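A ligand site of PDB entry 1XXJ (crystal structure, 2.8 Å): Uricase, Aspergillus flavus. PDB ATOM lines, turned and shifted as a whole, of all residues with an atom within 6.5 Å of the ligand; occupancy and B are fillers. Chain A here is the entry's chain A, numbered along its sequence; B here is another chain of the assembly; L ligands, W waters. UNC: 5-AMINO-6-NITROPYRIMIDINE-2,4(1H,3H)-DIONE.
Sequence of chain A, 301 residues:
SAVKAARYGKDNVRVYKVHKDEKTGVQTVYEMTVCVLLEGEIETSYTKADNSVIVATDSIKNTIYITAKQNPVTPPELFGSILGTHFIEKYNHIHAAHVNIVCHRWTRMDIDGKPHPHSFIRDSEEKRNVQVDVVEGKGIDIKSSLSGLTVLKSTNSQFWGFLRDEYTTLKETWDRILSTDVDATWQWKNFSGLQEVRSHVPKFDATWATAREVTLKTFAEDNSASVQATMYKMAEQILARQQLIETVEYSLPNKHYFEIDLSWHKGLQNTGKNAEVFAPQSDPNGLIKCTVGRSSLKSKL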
ATOM      1  N   SER A 157     -25.853  15.598 -29.997  1.00  0.00           N
ATOM      2  CA  SER A 157     -24.575  16.202 -29.730  1.00  0.00           C
ATOM      3  C   SER A 157     -24.915  17.612 -29.375  1.00  0.00           C
ATOM      4  O   SER A 157     -25.696  18.261 -30.072  1.00  0.00           O
ATOM      5  CB  SER A 157     -23.663  16.184 -30.973  1.00  0.00           C
ATOM      6  OG  SER A 157     -22.461  16.935 -30.754  1.00  0.00           O
ATOM      7  N   GLN A 158     -24.347  18.106 -28.289  1.00  0.00           N
ATOM      8  CA  GLN A 158     -24.609  19.481 -27.882  1.00  0.00           C
ATOM      9  C   GLN A 158     -23.330  20.101 -27.472  1.00  0.00           C
ATOM     10  O   GLN A 158     -22.382  19.424 -27.170  1.00  0.00           O
ATOM     11  CB  GLN A 158     -25.613  19.555 -26.706  1.00  0.00           C
ATOM     12  CG  GLN A 158     -26.081  18.209 -26.174  1.00  0.00           C
ATOM     13  CD  GLN A 158     -27.288  18.341 -25.265  1.00  0.00           C
ATOM     14  OE1 GLN A 158     -27.217  19.012 -24.214  1.00  0.00           O
ATOM     15  NE2 GLN A 158     -28.404  17.767 -25.689  1.00  0.00           N
ATOM     16  N   PHE A 159     -23.306  21.405 -27.419  1.00  0.00           N
ATOM     17  CA  PHE A 159     -22.128  22.089 -26.937  1.00  0.00           C
ATOM     18  C   PHE A 159     -22.539  23.424 -26.348  1.00  0.00           C
ATOM     19  O   PHE A 159     -22.832  24.386 -27.084  1.00  0.00           O
ATOM     20  CB  PHE A 159     -21.072  22.249 -28.043  1.00  0.00           C
ATOM     21  CG  PHE A 159     -19.746  22.801 -27.552  1.00  0.00           C
ATOM     22  CD1 PHE A 159     -19.039  22.166 -26.562  1.00  0.00           C
ATOM     23  CD2 PHE A 159     -19.199  23.938 -28.130  1.00  0.00           C
ATOM     24  CE1 PHE A 159     -17.828  22.665 -26.139  1.00  0.00           C
ATOM     25  CE2 PHE A 159     -17.985  24.446 -27.718  1.00  0.00           C
ATOM     26  CZ  PHE A 159     -17.300  23.804 -26.722  1.00  0.00           C
ATOM     27  N   LEU A 170     -19.494  32.318 -30.281  1.00  0.00           N
ATOM     28  CA  LEU A 170     -20.117  31.059 -30.587  1.00  0.00           C
ATOM     29  C   LEU A 170     -21.325  30.799 -29.735  1.00  0.00           C
ATOM     30  O   LEU A 170     -21.223  30.713 -28.516  1.00  0.00           O
ATOM     31  CB  LEU A 170     -19.117  29.899 -30.441  1.00  0.00           C
ATOM     32  CG  LEU A 170     -19.681  28.477 -30.588  1.00  0.00           C
ATOM     33  CD1 LEU A 170     -19.928  28.132 -32.022  1.00  0.00           C
ATOM     34  CD2 LEU A 170     -18.778  27.450 -29.935  1.00  0.00           C
ATOM     35  N   ARG A 176     -26.669  19.640 -32.503  1.00  0.00           N
ATOM     36  CA  ARG A 176     -25.755  19.977 -33.570  1.00  0.00           C
ATOM     37  C   ARG A 176     -25.287  18.699 -34.207  1.00  0.00           C
ATOM     38  O   ARG A 176     -25.420  17.608 -33.612  1.00  0.00           O
ATOM     39  CB  ARG A 176     -24.554  20.715 -33.029  1.00  0.00           C
ATOM     40  CG  ARG A 176     -23.599  19.815 -32.270  1.00  0.00           C
ATOM     41  CD  ARG A 176     -22.490  20.632 -31.687  1.00  0.00           C
ATOM     42  NE  ARG A 176     -21.467  19.821 -31.050  1.00  0.00           N
ATOM     43  CZ  ARG A 176     -20.211  20.223 -30.882  1.00  0.00           C
ATOM     44  NH1 ARG A 176     -19.845  21.429 -31.260  1.00  0.00           N
ATOM     45  NH2 ARG A 176     -19.328  19.403 -30.314  1.00  0.00           N
ATOM     46  N   LEU A 178     -22.370  16.258 -35.421  1.00  0.00           N
ATOM     47  CA  LEU A 178     -21.018  15.892 -35.018  1.00  0.00           C
ATOM     48  C   LEU A 178     -20.468  14.955 -36.121  1.00  0.00           C
ATOM     49  O   LEU A 178     -21.138  13.985 -36.530  1.00  0.00           O
ATOM     50  CB  LEU A 178     -20.966  15.221 -33.642  1.00  0.00           C
ATOM     51  CG  LEU A 178     -19.534  15.099 -33.053  1.00  0.00           C
ATOM     52  CD1 LEU A 178     -18.972  16.485 -32.778  1.00  0.00           C
ATOM     53  CD2 LEU A 178     -19.488  14.280 -31.822  1.00  0.00           C
ATOM     54  N   SER A 224     -23.663  13.365 -26.709  1.00  0.00           N
ATOM     55  CA  SER A 224     -22.426  14.109 -26.512  1.00  0.00           C
ATOM     56  C   SER A 224     -22.486  15.496 -25.849  1.00  0.00           C
ATOM     57  O   SER A 224     -23.157  16.416 -26.346  1.00  0.00           O
ATOM     58  CB  SER A 224     -21.620  14.167 -27.840  1.00  0.00           C
ATOM     59  OG  SER A 224     -20.353  14.783 -27.659  1.00  0.00           O
ATOM     60  N   ALA A 225     -21.720  15.657 -24.756  1.00  0.00           N
ATOM     61  CA  ALA A 225     -21.625  16.956 -24.049  1.00  0.00           C
ATOM     62  C   ALA A 225     -20.493  17.802 -24.671  1.00  0.00           C
ATOM     63  O   ALA A 225     -20.555  19.044 -24.730  1.00  0.00           O
ATOM     64  CB  ALA A 225     -21.383  16.740 -22.555  1.00  0.00           C
ATOM     65  N   SER A 226     -19.456  17.092 -25.160  1.00  0.00           N
ATOM     66  CA  SER A 226     -18.292  17.652 -25.848  1.00  0.00           C
ATOM     67  C   SER A 226     -17.582  16.475 -26.543  1.00  0.00           C
ATOM     68  O   SER A 226     -17.771  15.307 -26.154  1.00  0.00           O
ATOM     69  CB  SER A 226     -17.330  18.344 -24.854  1.00  0.00           C
ATOM     70  OG  SER A 226     -17.094  17.531 -23.688  1.00  0.00           O
ATOM     71  N   VAL A 227     -16.776  16.772 -27.565  1.00  0.00           N
ATOM     72  CA  VAL A 227     -16.010  15.742 -28.248  1.00  0.00           C
ATOM     73  C   VAL A 227     -15.115  15.100 -27.178  1.00  0.00           C
ATOM     74  O   VAL A 227     -14.972  13.879 -27.106  1.00  0.00           O
ATOM     75  CB  VAL A 227     -15.085  16.362 -29.314  1.00  0.00           C
ATOM     76  CG1 VAL A 227     -14.336  15.272 -30.095  1.00  0.00           C
ATOM     77  CG2 VAL A 227     -15.874  17.289 -30.249  1.00  0.00           C
ATOM     78  N   GLN A 228     -14.546  15.990 -26.355  1.00  0.00           N
ATOM     79  CA  GLN A 228     -13.659  15.639 -25.236  1.00  0.00           C
ATOM     80  C   GLN A 228     -14.249  14.555 -24.344  1.00  0.00           C
ATOM     81  O   GLN A 228     -13.552  13.611 -23.931  1.00  0.00           O
ATOM     82  CB  GLN A 228     -13.437  16.870 -24.348  1.00  0.00           C
ATOM     83  CG  GLN A 228     -12.599  17.973 -24.955  1.00  0.00           C
ATOM     84  CD  GLN A 228     -13.388  18.819 -25.889  1.00  0.00           C
ATOM     85  OE1 GLN A 228     -13.020  19.965 -26.165  1.00  0.00           O
ATOM     86  NE2 GLN A 228     -14.473  18.256 -26.442  1.00  0.00           N
ATOM     87  N   ASN A 254     -12.628  17.938 -35.359  1.00  0.00           N
ATOM     88  CA  ASN A 254     -14.048  18.186 -35.284  1.00  0.00           C
ATOM     89  C   ASN A 254     -14.419  18.921 -36.580  1.00  0.00           C
ATOM     90  O   ASN A 254     -14.070  20.092 -36.760  1.00  0.00           O
ATOM     91  CB  ASN A 254     -14.351  19.035 -34.035  1.00  0.00           C
ATOM     92  CG  ASN A 254     -15.860  19.386 -33.880  1.00  0.00           C
ATOM     93  OD1 ASN A 254     -16.741  18.697 -34.404  1.00  0.00           O
ATOM     94  ND2 ASN A 254     -16.145  20.477 -33.148  1.00  0.00           N
ATOM     95  N   HIS A 256     -16.728  20.832 -38.845  1.00  0.00           N
ATOM     96  CA  HIS A 256     -17.959  21.648 -38.731  1.00  0.00           C
ATOM     97  C   HIS A 256     -18.917  21.729 -39.898  1.00  0.00           C
ATOM     98  O   HIS A 256     -18.536  21.804 -41.068  1.00  0.00           O
ATOM     99  CB  HIS A 256     -17.642  23.045 -38.229  1.00  0.00           C
ATOM    100  CG  HIS A 256     -16.553  23.081 -37.217  1.00  0.00           C
ATOM    101  ND1 HIS A 256     -16.627  22.374 -36.037  1.00  0.00           N
ATOM    102  CD2 HIS A 256     -15.350  23.674 -37.222  1.00  0.00           C
ATOM    103  CE1 HIS A 256     -15.502  22.539 -35.356  1.00  0.00           C
ATOM    104  NE2 HIS A 256     -14.711  23.333 -36.052  1.00  0.00           N
ATOM    105  N   GLY A 286     -11.822  22.082 -35.547  1.00  0.00           N
ATOM    106  CA  GLY A 286     -11.382  21.872 -34.199  1.00  0.00           C
ATOM    107  C   GLY A 286     -10.630  20.564 -34.226  1.00  0.00           C
ATOM    108  O   GLY A 286     -10.962  19.644 -35.017  1.00  0.00           O
ATOM    109  N   ILE A 288      -9.132  17.845 -31.412  1.00  0.00           N
ATOM    110  CA  ILE A 288      -9.168  17.485 -29.996  1.00  0.00           C
ATOM    111  C   ILE A 288      -8.450  16.154 -29.739  1.00  0.00           C
ATOM    112  O   ILE A 288      -8.879  15.093 -30.209  1.00  0.00           O
ATOM    113  CB  ILE A 288     -10.652  17.333 -29.515  1.00  0.00           C
ATOM    114  CG1 ILE A 288     -11.315  18.690 -29.311  1.00  0.00           C
ATOM    115  CG2 ILE A 288     -10.716  16.556 -28.230  1.00  0.00           C
ATOM    116  CD1 ILE A 288     -11.957  19.258 -30.536  1.00  0.00           C
ATOM    117  N   TYR B   8      -6.230  20.628 -27.303  1.00  0.00           N
ATOM    118  CA  TYR B   8      -7.384  20.805 -28.142  1.00  0.00           C
ATOM    119  C   TYR B   8      -7.221  22.194 -28.671  1.00  0.00           C
ATOM    120  O   TYR B   8      -6.648  23.075 -28.011  1.00  0.00           O
ATOM    121  CB  TYR B   8      -8.684  20.644 -27.334  1.00  0.00           C
ATOM    122  CG  TYR B   8      -9.143  21.889 -26.619  1.00  0.00           C
ATOM    123  CD1 TYR B   8      -8.742  22.168 -25.309  1.00  0.00           C
ATOM    124  CD2 TYR B   8      -9.913  22.827 -27.263  1.00  0.00           C
ATOM    125  CE1 TYR B   8      -9.130  23.322 -24.679  1.00  0.00           C
ATOM    126  CE2 TYR B   8     -10.287  23.987 -26.652  1.00  0.00           C
ATOM    127  CZ  TYR B   8      -9.895  24.235 -25.360  1.00  0.00           C
ATOM    128  OH  TYR B   8     -10.289  25.408 -24.744  1.00  0.00           O
ATOM    129  N   GLY B   9      -7.646  22.417 -29.894  1.00  0.00           N
ATOM    130  CA  GLY B   9      -7.475  23.720 -30.460  1.00  0.00           C
ATOM    131  C   GLY B   9      -8.144  23.761 -31.788  1.00  0.00           C
ATOM    132  O   GLY B   9      -9.061  22.974 -32.058  1.00  0.00           O
ATOM    133  N   LYS B  10      -7.712  24.704 -32.600  1.00  0.00           N
ATOM    134  CA  LYS B  10      -8.260  24.841 -33.917  1.00  0.00           C
ATOM    135  C   LYS B  10      -7.127  24.580 -34.885  1.00  0.00           C
ATOM    136  O   LYS B  10      -5.984  24.930 -34.608  1.00  0.00           O
ATOM    137  CB  LYS B  10      -8.837  26.240 -34.125  1.00  0.00           C
ATOM    138  CG  LYS B  10      -9.857  26.313 -35.252  1.00  0.00           C
ATOM    139  CD  LYS B  10     -11.111  25.477 -34.954  1.00  0.00           C
ATOM    140  CE  LYS B  10     -12.360  26.347 -35.007  1.00  0.00           C
ATOM    141  NZ  LYS B  10     -13.630  25.599 -35.107  1.00  0.00           N
ATOM    142  N   ILE B  54     -13.440  24.832 -20.914  1.00  0.00           N
ATOM    143  CA  ILE B  54     -13.177  24.914 -22.336  1.00  0.00           C
ATOM    144  C   ILE B  54     -13.271  26.282 -23.018  1.00  0.00           C
ATOM    145  O   ILE B  54     -14.340  26.880 -23.097  1.00  0.00           O
ATOM    146  CB  ILE B  54     -14.019  23.944 -23.131  1.00  0.00           C
ATOM    147  CG1 ILE B  54     -13.706  22.514 -22.726  1.00  0.00           C
ATOM    148  CG2 ILE B  54     -13.759  24.141 -24.622  1.00  0.00           C
ATOM    149  CD1 ILE B  54     -14.882  21.584 -22.874  1.00  0.00           C
ATOM    150  N   VAL B  55     -12.150  26.732 -23.565  1.00  0.00           N
ATOM    151  CA  VAL B  55     -12.144  27.939 -24.367  1.00  0.00           C
ATOM    152  C   VAL B  55     -12.512  27.373 -25.742  1.00  0.00           C
ATOM    153  O   VAL B  55     -11.862  26.443 -26.227  1.00  0.00           O
ATOM    154  CB  VAL B  55     -10.713  28.583 -24.446  1.00  0.00           C
ATOM    155  CG1 VAL B  55     -10.762  29.871 -25.230  1.00  0.00           C
ATOM    156  CG2 VAL B  55     -10.186  28.832 -23.064  1.00  0.00           C
ATOM    157  N   ALA B  56     -13.600  27.857 -26.303  1.00  0.00           N
ATOM    158  CA  ALA B  56     -14.092  27.332 -27.565  1.00  0.00           C
ATOM    159  C   ALA B  56     -13.094  27.478 -28.691  1.00  0.00           C
ATOM    160  O   ALA B  56     -12.489  28.531 -28.875  1.00  0.00           O
ATOM    161  CB  ALA B  56     -15.434  27.967 -27.922  1.00  0.00           C
ATOM    162  N   THR B  57     -12.943  26.402 -29.463  1.00  0.00           N
ATOM    163  CA  THR B  57     -12.026  26.365 -30.600  1.00  0.00           C
ATOM    164  C   THR B  57     -12.365  27.447 -31.579  1.00  0.00           C
ATOM    165  O   THR B  57     -11.508  27.922 -32.318  1.00  0.00           O
ATOM    166  CB  THR B  57     -12.064  24.985 -31.326  1.00  0.00           C
ATOM    167  OG1 THR B  57     -13.282  24.854 -32.082  1.00  0.00           O
ATOM    168  CG2 THR B  57     -11.931  23.825 -30.295  1.00  0.00           C
ATOM    169  N   ASP B  58     -13.626  27.879 -31.570  1.00  0.00           N
ATOM    170  CA  ASP B  58     -14.085  28.962 -32.429  1.00  0.00           C
ATOM    171  C   ASP B  58     -13.474  30.242 -31.871  1.00  0.00           C
ATOM    172  O   ASP B  58     -13.035  31.133 -32.601  1.00  0.00           O
ATOM    173  CB  ASP B  58     -15.600  29.037 -32.390  1.00  0.00           C
ATOM    174  CG  ASP B  58     -16.183  29.927 -33.484  1.00  0.00           C
ATOM    175  OD1 ASP B  58     -16.237  29.464 -34.644  1.00  0.00           O
ATOM    176  OD2 ASP B  58     -16.627  31.062 -33.172  1.00  0.00           O
ATOM    177  N   SER B  59     -13.431  30.309 -30.542  1.00  0.00           N
ATOM    178  CA  SER B  59     -12.885  31.472 -29.846  1.00  0.00           C
ATOM    179  C   SER B  59     -11.423  31.608 -30.236  1.00  0.00           C
ATOM    180  O   SER B  59     -10.966  32.716 -30.561  1.00  0.00           O
ATOM    181  CB  SER B  59     -13.013  31.289 -28.340  1.00  0.00           C
ATOM    182  OG  SER B  59     -14.369  31.394 -27.932  1.00  0.00           O
ATOM    183  N   ILE B  60     -10.700  30.493 -30.215  1.00  0.00           N
ATOM    184  CA  ILE B  60      -9.290  30.502 -30.618  1.00  0.00           C
ATOM    185  C   ILE B  60      -9.162  30.998 -32.056  1.00  0.00           C
ATOM    186  O   ILE B  60      -8.239  31.744 -32.397  1.00  0.00           O
ATOM    187  CB  ILE B  60      -8.696  29.171 -30.592  1.00  0.00           C
ATOM    188  CG1 ILE B  60      -8.484  28.700 -29.141  1.00  0.00           C
ATOM    189  CG2 ILE B  60      -7.412  29.203 -31.396  1.00  0.00           C
ATOM    190  CD1 ILE B  60      -8.775  27.249 -28.949  1.00  0.00           C
HETATM  191  OD2 UNC L   1     -17.437  23.768 -31.662  1.00  0.00           O
HETATM  192  N4  UNC L   1     -16.547  24.055 -30.831  1.00  0.00           N
HETATM  193  OD1 UNC L   1     -15.918  25.131 -30.786  1.00  0.00           O
HETATM  194  C4  UNC L   1     -16.198  22.939 -29.959  1.00  0.00           C
HETATM  195  N3  UNC L   1     -16.885  21.729 -29.996  1.00  0.00           N
HETATM  196  C2  UNC L   1     -16.408  20.694 -29.058  1.00  0.00           C
HETATM  197  O2  UNC L   1     -16.907  19.554 -28.974  1.00  0.00           O
HETATM  198  C5  UNC L   1     -15.114  23.288 -29.137  1.00  0.00           C
HETATM  199  N5  UNC L   1     -14.517  24.444 -29.141  1.00  0.00           N
HETATM  200  C6  UNC L   1     -14.591  22.271 -28.161  1.00  0.00           C
HETATM  201  O6  UNC L   1     -13.645  22.482 -27.390  1.00  0.00           O
HETATM  202  N1  UNC L   1     -15.297  21.032 -28.219  1.00  0.00           N
HETATM  203  O   HOH W   1     -14.261  22.613 -32.174  1.00  0.00           O
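The side-chain hydroxyl of Thr 57 of chain B lies within hydrogen-bond range of the side-chain amino group of Lys 10 of chain B, at 3.1 Å.
OG of Ser 224 lies within hydrogen-bond range of O of Ser 226 (3.0 Å).
A ring nitrogen (NE2) of His 256 lies close to the backbone carbonyl oxygen (O) of Asn 254, at 3.4 Å.
The backbone carbonyl oxygen (O) of Gly 286 sits at hydrogen-bond distance from the backbone NH (N) of Asn 254 (2.4 Å).
O of Ser 157 sits at hydrogen-bond distance from N of Arg 176 (3.0 Å).
The side-chain hydroxyl of Tyr 8 of chain B sits at hydrogen-bond distance from the backbone NH of Val 55 of chain B (2.6 Å).
Merely in contact with the ligand: Ile 54 of chain B, Phe 159, Ala 56 of chain B, Asp 58 of chain B, Tyr 8 of chain B, Leu 170 and Ser 226.
Within 4 Å of the ligand: Phe 159, Leu 170, Arg 176, Ser 226, Val 227, Gln 228, Asn 254, Tyr 8 of chain B, Ile 54 of chain B, Ala 56 of chain B, Thr 57 of chain B and Asp 58 of chain B.
Water W1 lies within hydrogen-bond range of OG1 of Thr 57 of chain B (2.4 Å), ND2 of Asn 254 (3.0 Å) and OD1 of the ligand (3.3 Å).
NH2 of Arg 176 sits at hydrogen-bond distance from O2 of the ligand, 2.8 Å away.
An oxygen (O2) of the ligand sits close to the backbone NH (N) of Val 227 (3.1 Å).
An oxygen (O6) of the ligand sits close to the side-chain amide oxygen (OE1) of Gln 228, at 2.9 Å.
The side-chain hydroxyl (OG1) of Thr 57 of chain B sits at hydrogen-bond distance from an oxygen (OD1) of the ligand (3.0 Å).
N of Thr 57 of chain B lies within hydrogen-bond range of OD1 of the ligand (3.5 Å).
A nitrogen (N3) of the ligand lies close to the side-chain amide nitrogen of Asn 254 (3.5 Å).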
